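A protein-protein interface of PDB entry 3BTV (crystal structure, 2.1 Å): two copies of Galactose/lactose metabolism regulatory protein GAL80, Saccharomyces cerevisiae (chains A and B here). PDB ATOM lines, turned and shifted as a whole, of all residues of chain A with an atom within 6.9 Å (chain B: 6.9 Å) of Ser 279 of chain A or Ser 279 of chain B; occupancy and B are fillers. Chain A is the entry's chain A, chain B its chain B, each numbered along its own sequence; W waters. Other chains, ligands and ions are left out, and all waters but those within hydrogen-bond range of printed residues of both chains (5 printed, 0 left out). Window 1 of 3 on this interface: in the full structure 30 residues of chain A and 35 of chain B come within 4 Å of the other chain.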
ATOM      1  N   SER A 178     -20.052 -12.763   9.547  1.00  0.00           N
ATOM      2  CA  SER A 178     -19.133 -13.507  10.410  1.00  0.00           C
ATOM      3  C   SER A 178     -19.170 -14.996  10.104  1.00  0.00           C
ATOM      4  O   SER A 178     -20.092 -15.496   9.440  1.00  0.00           O
ATOM      5  CB  SER A 178     -19.464 -13.259  11.882  1.00  0.00           C
ATOM      6  OG  SER A 178     -20.801 -13.651  12.169  1.00  0.00           O
ATOM      7  N   ILE A 179     -18.163 -15.702  10.593  1.00  0.00           N
ATOM      8  CA  ILE A 179     -17.996 -17.117  10.269  1.00  0.00           C
ATOM      9  C   ILE A 179     -17.508 -17.884  11.482  1.00  0.00           C
ATOM     10  O   ILE A 179     -16.604 -17.421  12.186  1.00  0.00           O
ATOM     11  CB  ILE A 179     -16.962 -17.287   9.142  1.00  0.00           C
ATOM     12  CG1 ILE A 179     -17.438 -16.575   7.870  1.00  0.00           C
ATOM     13  CG2 ILE A 179     -16.632 -18.793   8.913  1.00  0.00           C
ATOM     14  CD1 ILE A 179     -16.465 -16.703   6.678  1.00  0.00           C
ATOM     15  N   GLU A 180     -18.104 -19.048  11.725  1.00  0.00           N
ATOM     16  CA  GLU A 180     -17.631 -19.956  12.776  1.00  0.00           C
ATOM     17  C   GLU A 180     -17.357 -21.348  12.215  1.00  0.00           C
ATOM     18  O   GLU A 180     -18.100 -21.876  11.369  1.00  0.00           O
ATOM     19  CB  GLU A 180     -18.646 -20.091  13.932  1.00  0.00           C
ATOM     20  CG  GLU A 180     -18.844 -18.841  14.770  1.00  0.00           C
ATOM     21  CD  GLU A 180     -20.048 -18.042  14.339  1.00  0.00           C
ATOM     22  OE1 GLU A 180     -21.155 -18.632  14.316  1.00  0.00           O
ATOM     23  OE2 GLU A 180     -19.888 -16.833  14.034  1.00  0.00           O
ATOM     24  N   ILE A 181     -16.298 -21.956  12.716  1.00  0.00           N
ATOM     25  CA  ILE A 181     -15.886 -23.264  12.241  1.00  0.00           C
ATOM     26  C   ILE A 181     -15.545 -24.104  13.445  1.00  0.00           C
ATOM     27  O   ILE A 181     -14.849 -23.652  14.359  1.00  0.00           O
ATOM     28  CB  ILE A 181     -14.625 -23.211  11.396  1.00  0.00           C
ATOM     29  CG1 ILE A 181     -14.806 -22.251  10.219  1.00  0.00           C
ATOM     30  CG2 ILE A 181     -14.278 -24.621  10.887  1.00  0.00           C
ATOM     31  CD1 ILE A 181     -13.642 -22.283   9.264  1.00  0.00           C
ATOM     32  N   ALA A 182     -16.026 -25.333  13.435  1.00  0.00           N
ATOM     33  CA  ALA A 182     -15.715 -26.257  14.507  1.00  0.00           C
ATOM     34  C   ALA A 182     -15.405 -27.573  13.833  1.00  0.00           C
ATOM     35  O   ALA A 182     -16.167 -28.026  12.979  1.00  0.00           O
ATOM     36  CB  ALA A 182     -16.901 -26.371  15.436  1.00  0.00           C
ATOM     37  N   HIS A 264      -5.264 -29.712  20.148  1.00  0.00           N
ATOM     38  CA  HIS A 264      -6.279 -28.675  19.975  1.00  0.00           C
ATOM     39  C   HIS A 264      -5.760 -27.442  19.253  1.00  0.00           C
ATOM     40  O   HIS A 264      -4.608 -27.060  19.409  1.00  0.00           O
ATOM     41  CB  HIS A 264      -6.894 -28.273  21.319  1.00  0.00           C
ATOM     42  CG  HIS A 264      -8.313 -27.798  21.218  1.00  0.00           C
ATOM     43  ND1 HIS A 264      -8.646 -26.477  20.994  1.00  0.00           N
ATOM     44  CD2 HIS A 264      -9.488 -28.474  21.307  1.00  0.00           C
ATOM     45  CE1 HIS A 264      -9.964 -26.358  20.953  1.00  0.00           C
ATOM     46  NE2 HIS A 264     -10.497 -27.552  21.155  1.00  0.00           N
ATOM     47  N   LEU A 265      -6.621 -26.826  18.463  1.00  0.00           N
ATOM     48  CA  LEU A 265      -6.280 -25.567  17.811  1.00  0.00           C
ATOM     49  C   LEU A 265      -7.390 -24.571  18.040  1.00  0.00           C
ATOM     50  O   LEU A 265      -8.586 -24.848  17.763  1.00  0.00           O
ATOM     51  CB  LEU A 265      -6.048 -25.757  16.311  1.00  0.00           C
ATOM     52  CG  LEU A 265      -5.941 -24.447  15.501  1.00  0.00           C
ATOM     53  CD1 LEU A 265      -4.630 -23.625  15.768  1.00  0.00           C
ATOM     54  CD2 LEU A 265      -6.111 -24.724  14.011  1.00  0.00           C
ATOM     55  N   LEU A 266      -7.015 -23.419  18.581  1.00  0.00           N
ATOM     56  CA  LEU A 266      -7.910 -22.269  18.612  1.00  0.00           C
ATOM     57  C   LEU A 266      -7.401 -21.290  17.577  1.00  0.00           C
ATOM     58  O   LEU A 266      -6.212 -20.956  17.570  1.00  0.00           O
ATOM     59  CB  LEU A 266      -7.885 -21.590  19.977  1.00  0.00           C
ATOM     60  CG  LEU A 266      -8.401 -22.363  21.198  1.00  0.00           C
ATOM     61  CD1 LEU A 266      -8.200 -21.496  22.426  1.00  0.00           C
ATOM     62  CD2 LEU A 266      -9.898 -22.756  21.064  1.00  0.00           C
ATOM     63  N   PHE A 267      -8.283 -20.816  16.711  1.00  0.00           N
ATOM     64  CA  PHE A 267      -7.852 -19.931  15.634  1.00  0.00           C
ATOM     65  C   PHE A 267      -8.921 -18.889  15.427  1.00  0.00           C
ATOM     66  O   PHE A 267     -10.119 -19.202  15.377  1.00  0.00           O
ATOM     67  CB  PHE A 267      -7.587 -20.730  14.349  1.00  0.00           C
ATOM     68  CG  PHE A 267      -7.421 -19.868  13.100  1.00  0.00           C
ATOM     69  CD1 PHE A 267      -6.163 -19.566  12.628  1.00  0.00           C
ATOM     70  CD2 PHE A 267      -8.522 -19.415  12.393  1.00  0.00           C
ATOM     71  CE1 PHE A 267      -5.999 -18.788  11.460  1.00  0.00           C
ATOM     72  CE2 PHE A 267      -8.376 -18.639  11.243  1.00  0.00           C
ATOM     73  CZ  PHE A 267      -7.092 -18.343  10.776  1.00  0.00           C
ATOM     74  N   GLN A 268      -8.501 -17.634  15.358  1.00  0.00           N
ATOM     75  CA  GLN A 268      -9.439 -16.557  15.039  1.00  0.00           C
ATOM     76  C   GLN A 268      -8.758 -15.571  14.135  1.00  0.00           C
ATOM     77  O   GLN A 268      -7.550 -15.385  14.238  1.00  0.00           O
ATOM     78  CB  GLN A 268      -9.971 -15.872  16.304  1.00  0.00           C
ATOM     79  CG  GLN A 268      -8.918 -15.167  17.113  1.00  0.00           C
ATOM     80  CD  GLN A 268      -9.420 -14.682  18.465  1.00  0.00           C
ATOM     81  OE1 GLN A 268      -8.802 -13.815  19.095  1.00  0.00           O
ATOM     82  NE2 GLN A 268     -10.534 -15.239  18.921  1.00  0.00           N
ATOM     83  N   GLY A 269      -9.512 -14.967  13.228  1.00  0.00           N
ATOM     84  CA  GLY A 269      -8.911 -14.030  12.294  1.00  0.00           C
ATOM     85  C   GLY A 269      -9.945 -13.241  11.519  1.00  0.00           C
ATOM     86  O   GLY A 269     -11.168 -13.379  11.724  1.00  0.00           O
ATOM     87  N   VAL A 276     -14.008  -9.655   7.688  1.00  0.00           N
ATOM     88  CA  VAL A 276     -14.967 -10.614   8.299  1.00  0.00           C
ATOM     89  C   VAL A 276     -14.349 -11.397   9.456  1.00  0.00           C
ATOM     90  O   VAL A 276     -13.342 -12.076   9.290  1.00  0.00           O
ATOM     91  CB  VAL A 276     -15.459 -11.649   7.276  1.00  0.00           C
ATOM     92  CG1 VAL A 276     -16.438 -12.692   7.943  1.00  0.00           C
ATOM     93  CG2 VAL A 276     -16.094 -10.964   6.083  1.00  0.00           C
ATOM     94  N   PRO A 277     -14.953 -11.304  10.638  1.00  0.00           N
ATOM     95  CA  PRO A 277     -14.543 -12.117  11.791  1.00  0.00           C
ATOM     96  C   PRO A 277     -14.743 -13.629  11.545  1.00  0.00           C
ATOM     97  O   PRO A 277     -15.829 -14.068  11.181  1.00  0.00           O
ATOM     98  CB  PRO A 277     -15.484 -11.647  12.912  1.00  0.00           C
ATOM     99  CG  PRO A 277     -16.145 -10.413  12.402  1.00  0.00           C
ATOM    100  CD  PRO A 277     -16.134 -10.478  10.924  1.00  0.00           C
ATOM    101  N   VAL A 278     -13.687 -14.404  11.755  1.00  0.00           N
ATOM    102  CA  VAL A 278     -13.714 -15.855  11.613  1.00  0.00           C
ATOM    103  C   VAL A 278     -13.251 -16.446  12.934  1.00  0.00           C
ATOM    104  O   VAL A 278     -12.201 -16.080  13.452  1.00  0.00           O
ATOM    105  CB  VAL A 278     -12.774 -16.359  10.501  1.00  0.00           C
ATOM    106  CG1 VAL A 278     -12.832 -17.900  10.416  1.00  0.00           C
ATOM    107  CG2 VAL A 278     -13.098 -15.703   9.146  1.00  0.00           C
ATOM    108  N   SER A 279     -14.061 -17.326  13.505  1.00  0.00           N
ATOM    109  CA  SER A 279     -13.698 -17.994  14.752  1.00  0.00           C
ATOM    110  C   SER A 279     -13.656 -19.514  14.545  1.00  0.00           C
ATOM    111  O   SER A 279     -14.600 -20.099  14.032  1.00  0.00           O
ATOM    112  CB  SER A 279     -14.733 -17.660  15.835  1.00  0.00           C
ATOM    113  OG  SER A 279     -14.440 -18.376  17.021  1.00  0.00           O
ATOM    114  N   CYS A 280     -12.593 -20.147  15.015  1.00  0.00           N
ATOM    115  CA  CYS A 280     -12.394 -21.554  14.725  1.00  0.00           C
ATOM    116  C   CYS A 280     -11.809 -22.373  15.879  1.00  0.00           C
ATOM    117  O   CYS A 280     -10.862 -21.950  16.548  1.00  0.00           O
ATOM    118  CB  CYS A 280     -11.519 -21.687  13.489  1.00  0.00           C
ATOM    119  SG  CYS A 280     -11.013 -23.352  13.173  1.00  0.00           S
ATOM    120  N   SER A 281     -12.378 -23.556  16.100  1.00  0.00           N
ATOM    121  CA  SER A 281     -11.920 -24.441  17.170  1.00  0.00           C
ATOM    122  C   SER A 281     -11.837 -25.868  16.625  1.00  0.00           C
ATOM    123  O   SER A 281     -12.832 -26.426  16.162  1.00  0.00           O
ATOM    124  CB  SER A 281     -12.905 -24.397  18.344  1.00  0.00           C
ATOM    125  OG  SER A 281     -12.470 -25.212  19.417  1.00  0.00           O
ATOM    126  N   SER B 178     -12.322 -29.017  26.553  1.00  0.00           N
ATOM    127  CA  SER B 178     -12.431 -27.769  25.774  1.00  0.00           C
ATOM    128  C   SER B 178     -13.807 -27.142  25.900  1.00  0.00           C
ATOM    129  O   SER B 178     -14.760 -27.800  26.340  1.00  0.00           O
ATOM    130  CB  SER B 178     -12.102 -28.021  24.291  1.00  0.00           C
ATOM    131  OG  SER B 178     -13.049 -28.869  23.686  1.00  0.00           O
ATOM    132  N   ILE B 179     -13.914 -25.873  25.513  1.00  0.00           N
ATOM    133  CA  ILE B 179     -15.168 -25.107  25.670  1.00  0.00           C
ATOM    134  C   ILE B 179     -15.432 -24.186  24.482  1.00  0.00           C
ATOM    135  O   ILE B 179     -14.527 -23.502  24.019  1.00  0.00           O
ATOM    136  CB  ILE B 179     -15.088 -24.212  26.937  1.00  0.00           C
ATOM    137  CG1 ILE B 179     -14.822 -25.063  28.195  1.00  0.00           C
ATOM    138  CG2 ILE B 179     -16.324 -23.321  27.073  1.00  0.00           C
ATOM    139  CD1 ILE B 179     -14.696 -24.250  29.471  1.00  0.00           C
ATOM    140  N   GLU B 180     -16.664 -24.142  23.990  1.00  0.00           N
ATOM    141  CA  GLU B 180     -17.029 -23.116  22.998  1.00  0.00           C
ATOM    142  C   GLU B 180     -18.218 -22.304  23.451  1.00  0.00           C
ATOM    143  O   GLU B 180     -19.192 -22.822  24.013  1.00  0.00           O
ATOM    144  CB  GLU B 180     -17.326 -23.721  21.614  1.00  0.00           C
ATOM    145  CG  GLU B 180     -16.119 -24.420  20.961  1.00  0.00           C
ATOM    146  CD  GLU B 180     -15.943 -25.841  21.462  1.00  0.00           C
ATOM    147  OE1 GLU B 180     -16.986 -26.504  21.637  1.00  0.00           O
ATOM    148  OE2 GLU B 180     -14.784 -26.291  21.678  1.00  0.00           O
ATOM    149  N   ILE B 181     -18.158 -21.022  23.161  1.00  0.00           N
ATOM    150  CA  ILE B 181     -19.252 -20.132  23.486  1.00  0.00           C
ATOM    151  C   ILE B 181     -19.652 -19.320  22.266  1.00  0.00           C
ATOM    152  O   ILE B 181     -18.810 -18.732  21.598  1.00  0.00           O
ATOM    153  CB  ILE B 181     -18.842 -19.178  24.595  1.00  0.00           C
ATOM    154  CG1 ILE B 181     -18.462 -19.973  25.842  1.00  0.00           C
ATOM    155  CG2 ILE B 181     -19.969 -18.183  24.882  1.00  0.00           C
ATOM    156  CD1 ILE B 181     -18.026 -19.090  26.998  1.00  0.00           C
ATOM    157  N   ALA B 182     -20.941 -19.289  21.981  1.00  0.00           N
ATOM    158  CA  ALA B 182     -21.466 -18.458  20.907  1.00  0.00           C
ATOM    159  C   ALA B 182     -22.635 -17.676  21.471  1.00  0.00           C
ATOM    160  O   ALA B 182     -23.499 -18.246  22.138  1.00  0.00           O
ATOM    161  CB  ALA B 182     -21.927 -19.319  19.768  1.00  0.00           C
ATOM    162  N   HIS B 264     -18.885  -6.855  17.183  1.00  0.00           N
ATOM    163  CA  HIS B 264     -18.444  -8.260  17.246  1.00  0.00           C
ATOM    164  C   HIS B 264     -17.245  -8.429  18.145  1.00  0.00           C
ATOM    165  O   HIS B 264     -16.383  -7.557  18.213  1.00  0.00           O
ATOM    166  CB  HIS B 264     -18.090  -8.806  15.868  1.00  0.00           C
ATOM    167  CG  HIS B 264     -18.287 -10.283  15.739  1.00  0.00           C
ATOM    168  ND1 HIS B 264     -17.317 -11.201  16.087  1.00  0.00           N
ATOM    169  CD2 HIS B 264     -19.338 -11.006  15.290  1.00  0.00           C
ATOM    170  CE1 HIS B 264     -17.763 -12.424  15.858  1.00  0.00           C
ATOM    171  NE2 HIS B 264     -18.985 -12.335  15.354  1.00  0.00           N
ATOM    172  N   LEU B 265     -17.202  -9.563  18.829  1.00  0.00           N
ATOM    173  CA  LEU B 265     -16.081  -9.911  19.673  1.00  0.00           C
ATOM    174  C   LEU B 265     -15.643 -11.329  19.337  1.00  0.00           C
ATOM    175  O   LEU B 265     -16.466 -12.266  19.326  1.00  0.00           O
ATOM    176  CB  LEU B 265     -16.463  -9.824  21.161  1.00  0.00           C
ATOM    177  CG  LEU B 265     -15.430 -10.435  22.133  1.00  0.00           C
ATOM    178  CD1 LEU B 265     -14.154  -9.612  22.190  1.00  0.00           C
ATOM    179  CD2 LEU B 265     -15.994 -10.623  23.534  1.00  0.00           C
ATOM    180  N   LEU B 266     -14.357 -11.485  19.054  1.00  0.00           N
ATOM    181  CA  LEU B 266     -13.741 -12.813  18.963  1.00  0.00           C
ATOM    182  C   LEU B 266     -12.864 -12.925  20.174  1.00  0.00           C
ATOM    183  O   LEU B 266     -12.068 -12.031  20.451  1.00  0.00           O
ATOM    184  CB  LEU B 266     -12.874 -12.972  17.712  1.00  0.00           C
ATOM    185  CG  LEU B 266     -13.542 -12.838  16.342  1.00  0.00           C
ATOM    186  CD1 LEU B 266     -12.494 -12.880  15.239  1.00  0.00           C
ATOM    187  CD2 LEU B 266     -14.585 -13.927  16.128  1.00  0.00           C
ATOM    188  N   PHE B 267     -13.009 -14.010  20.915  1.00  0.00           N
ATOM    189  CA  PHE B 267     -12.226 -14.165  22.130  1.00  0.00           C
ATOM    190  C   PHE B 267     -11.792 -15.601  22.266  1.00  0.00           C
ATOM    191  O   PHE B 267     -12.599 -16.522  22.130  1.00  0.00           O
ATOM    192  CB  PHE B 267     -13.048 -13.723  23.345  1.00  0.00           C
ATOM    193  CG  PHE B 267     -12.444 -14.120  24.679  1.00  0.00           C
ATOM    194  CD1 PHE B 267     -11.724 -13.208  25.436  1.00  0.00           C
ATOM    195  CD2 PHE B 267     -12.627 -15.397  25.186  1.00  0.00           C
ATOM    196  CE1 PHE B 267     -11.192 -13.568  26.661  1.00  0.00           C
ATOM    197  CE2 PHE B 267     -12.092 -15.766  26.408  1.00  0.00           C
ATOM    198  CZ  PHE B 267     -11.378 -14.856  27.151  1.00  0.00           C
ATOM    199  N   GLN B 268     -10.512 -15.806  22.526  1.00  0.00           N
ATOM    200  CA  GLN B 268     -10.042 -17.169  22.746  1.00  0.00           C
ATOM    201  C   GLN B 268      -9.049 -17.134  23.884  1.00  0.00           C
ATOM    202  O   GLN B 268      -8.376 -16.129  24.097  1.00  0.00           O
ATOM    203  CB  GLN B 268      -9.444 -17.772  21.470  1.00  0.00           C
ATOM    204  CG  GLN B 268      -8.153 -17.103  20.993  1.00  0.00           C
ATOM    205  CD  GLN B 268      -7.719 -17.578  19.607  1.00  0.00           C
ATOM    206  OE1 GLN B 268      -6.573 -17.382  19.180  1.00  0.00           O
ATOM    207  NE2 GLN B 268      -8.640 -18.200  18.900  1.00  0.00           N
ATOM    208  N   GLY B 269      -8.978 -18.208  24.650  1.00  0.00           N
ATOM    209  CA  GLY B 269      -8.092 -18.224  25.789  1.00  0.00           C
ATOM    210  C   GLY B 269      -8.010 -19.568  26.453  1.00  0.00           C
ATOM    211  O   GLY B 269      -8.636 -20.540  26.008  1.00  0.00           O
ATOM    212  N   VAL B 276      -7.299 -25.268  29.765  1.00  0.00           N
ATOM    213  CA  VAL B 276      -8.423 -25.606  28.873  1.00  0.00           C
ATOM    214  C   VAL B 276      -8.621 -24.563  27.775  1.00  0.00           C
ATOM    215  O   VAL B 276      -8.776 -23.380  28.065  1.00  0.00           O
ATOM    216  CB  VAL B 276      -9.755 -25.726  29.651  1.00  0.00           C
ATOM    217  CG1 VAL B 276     -10.930 -26.072  28.704  1.00  0.00           C
ATOM    218  CG2 VAL B 276      -9.635 -26.758  30.771  1.00  0.00           C
ATOM    219  N   PRO B 277      -8.628 -25.005  26.512  1.00  0.00           N
ATOM    220  CA  PRO B 277      -8.941 -24.116  25.390  1.00  0.00           C
ATOM    221  C   PRO B 277     -10.394 -23.635  25.446  1.00  0.00           C
ATOM    222  O   PRO B 277     -11.323 -24.440  25.576  1.00  0.00           O
ATOM    223  CB  PRO B 277      -8.753 -25.011  24.160  1.00  0.00           C
ATOM    224  CG  PRO B 277      -8.068 -26.254  24.650  1.00  0.00           C
ATOM    225  CD  PRO B 277      -8.367 -26.394  26.089  1.00  0.00           C
ATOM    226  N   VAL B 278     -10.585 -22.327  25.338  1.00  0.00           N
ATOM    227  CA  VAL B 278     -11.906 -21.727  25.303  1.00  0.00           C
ATOM    228  C   VAL B 278     -11.987 -20.863  24.056  1.00  0.00           C
ATOM    229  O   VAL B 278     -11.124 -20.008  23.833  1.00  0.00           O
ATOM    230  CB  VAL B 278     -12.133 -20.818  26.525  1.00  0.00           C
ATOM    231  CG1 VAL B 278     -13.495 -20.119  26.443  1.00  0.00           C
ATOM    232  CG2 VAL B 278     -11.992 -21.621  27.815  1.00  0.00           C
ATOM    233  N   SER B 279     -13.006 -21.090  23.239  1.00  0.00           N
ATOM    234  CA  SER B 279     -13.198 -20.312  22.017  1.00  0.00           C
ATOM    235  C   SER B 279     -14.551 -19.615  22.049  1.00  0.00           C
ATOM    236  O   SER B 279     -15.587 -20.250  22.296  1.00  0.00           O
ATOM    237  CB  SER B 279     -13.122 -21.237  20.792  1.00  0.00           C
ATOM    238  OG  SER B 279     -13.472 -20.543  19.601  1.00  0.00           O
ATOM    239  N   CYS B 280     -14.557 -18.331  21.728  1.00  0.00           N
ATOM    240  CA  CYS B 280     -15.762 -17.551  21.899  1.00  0.00           C
ATOM    241  C   CYS B 280     -16.020 -16.525  20.809  1.00  0.00           C
ATOM    242  O   CYS B 280     -15.127 -15.767  20.419  1.00  0.00           O
ATOM    243  CB  CYS B 280     -15.725 -16.859  23.252  1.00  0.00           C
ATOM    244  SG  CYS B 280     -17.074 -15.737  23.452  1.00  0.00           S
ATOM    245  N   SER B 281     -17.260 -16.494  20.334  1.00  0.00           N
ATOM    246  CA  SER B 281     -17.657 -15.531  19.307  1.00  0.00           C
ATOM    247  C   SER B 281     -18.975 -14.881  19.704  1.00  0.00           C
ATOM    248  O   SER B 281     -19.989 -15.571  19.874  1.00  0.00           O
ATOM    249  CB  SER B 281     -17.799 -16.234  17.958  1.00  0.00           C
ATOM    250  OG  SER B 281     -18.101 -15.322  16.924  1.00  0.00           O
HETATM  251  O   HOH W   1     -12.644 -16.879  18.608  1.00  0.00           O
HETATM  252  O   HOH W   2     -12.663 -24.798  21.967  1.00  0.00           O
HETATM  253  O   HOH W   3     -11.147 -19.536  18.620  1.00  0.00           O
HETATM  254  O   HOH W   4     -15.651 -20.573  18.035  1.00  0.00           O
HETATM  255  O   HOH W   5     -17.434 -15.414  14.203  1.00  0.00           O
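NE2 of Gln 268 of chain B sits close to N of Phe 267 of chain A (3.4 Å). The side-chain amide nitrogen (NE2) of Gln 268 of chain A sits close to the backbone NH (N) of Phe 267 of chain B (3.4 Å). The side-chain carboxylate of Glu 180 of chain B sits at hydrogen-bond distance from the side-chain hydroxyl of Ser 281 of chain A (3.4 Å).
N of Ile 179 of chain A lies within hydrogen-bond range of O of Pro 277 of chain A, 2.9 Å away. N of Ser 279 of chain A sits at hydrogen-bond distance from O of Ile 179 of chain A (2.9 Å). O of Ile 181 of chain A is in hydrogen-bond range of N of Ser 281 of chain A (3.0 Å). N of Cys 280 of chain A lies within hydrogen-bond range of O of Phe 267 of chain A (2.7 Å). The backbone NH (N) of Val 278 of chain A is in hydrogen-bond range of the backbone carbonyl oxygen (O) of Gly 269 of chain A, 2.7 Å away. The backbone carbonyl oxygen of Ile 181 of chain B sits at hydrogen-bond distance from the backbone NH of Ser 281 of chain B (3.0 Å).
ND1 of His 264 of chain A touches CB of Pro 277 of chain B, at 3.5 Å. C of Leu 266 of chain A touches NE2 of Gln 268 of chain B, at 3.6 Å. Gly 269 of chain B touches Leu 266 of chain A (O to CD1, 3.7 Å). Leu 266 of chain A touches Pro 277 of chain B. Leu 266 of chain A touches Val 278 of chain B (CD1 to O, 3.6 Å). Gln 268 of chain A touches Leu 266 of chain B (NE2 to CB, 3.5 Å). Gly 269 of chain A touches Leu 266 of chain B (O to CD1, 3.8 Å). Pro 277 of chain A touches His 264 of chain B. CD1 of Leu 266 of chain B touches CB of Pro 277 of chain A, at 3.98 Å. Ser 281 of chain B touches Ser 279 of chain A (CB to CB, 3.99 Å).
Of the printed residues of chain B, Glu 180 of chain A touches Ser 281 (3.7 Å). Of the printed residues of chain B, His 264 of chain A touches Ser 178 (3.6 Å) and Pro 277 (3.5 Å). Of the printed residues of chain B, Ser 279 of chain A touches Leu 266 (3.7 Å), Ser 279 (3.5 Å) and Ser 281 (3.99 Å). Printed residues of chain A within 4 Å of Ser 279 of chain B: Leu 266 and Ser 279.
Printed residues of chain B that touch a printed residue of chain A: Ser 178, Glu 180, His 264, Leu 266, Phe 267, Gln 268, Gly 269, Pro 277, Val 278, Ser 279 and Ser 281. Hydrophobic or aromatic side chains of chain B that line the printed part of chain A: His 264, Leu 266 and Pro 277. Among the printed residues, no Asp or Glu carboxylate lies within 4 Å of a Lys or Arg side-chain nitrogen of the other chain.
Glu 180 of chain A touches Ser 281 of chain B, and with the chains exchanged Ser 281 of chain A touches Glu 180 of chain B. His 264 of chain A touches Pro 277 of chain B, and with the chains exchanged Pro 277 of chain A touches His 264 of chain B. Leu 266 of chain A touches Ser 279 of chain B, and with the chains exchanged Ser 279 of chain A touches Leu 266 of chain B. Ser 279 of chain A touches Ser 281 of chain B, but with the chains exchanged Ser 281 of chain A does not touch Ser 279 of chain B (4.003 Å).
Water W2 lies within hydrogen-bond range of the side-chain hydroxyl (OG) of Ser 281 of chain A (2.6 Å), the side-chain carboxylate (OE2) of Glu 180 of chain B (2.6 Å) and the backbone carbonyl oxygen (O) of Ile 179 of chain B (3.1 Å). Water W4 lies within hydrogen-bond range of OG of Ser 279 of chain B (2.7 Å) and OG of Ser 279 of chain A (2.7 Å). Water W1 lies within hydrogen-bond range of NE2 of Gln 268 of chain A (2.7 Å), OG of Ser 279 of chain A (2.8 Å) and O of Cys 280 of chain B (3.3 Å). Water W3 lies within hydrogen-bond range of OG of Ser 279 of chain B, NE2 of Gln 268 of chain B, O of Cys 280 of chain A and O of Phe 267 of chain A. Water W5 lies within hydrogen-bond range of the side-chain hydroxyl of Ser 281 of chain B, the side-chain carboxylate of Glu 180 of chain A and the backbone carbonyl oxygen of Ile 179 of chain A.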
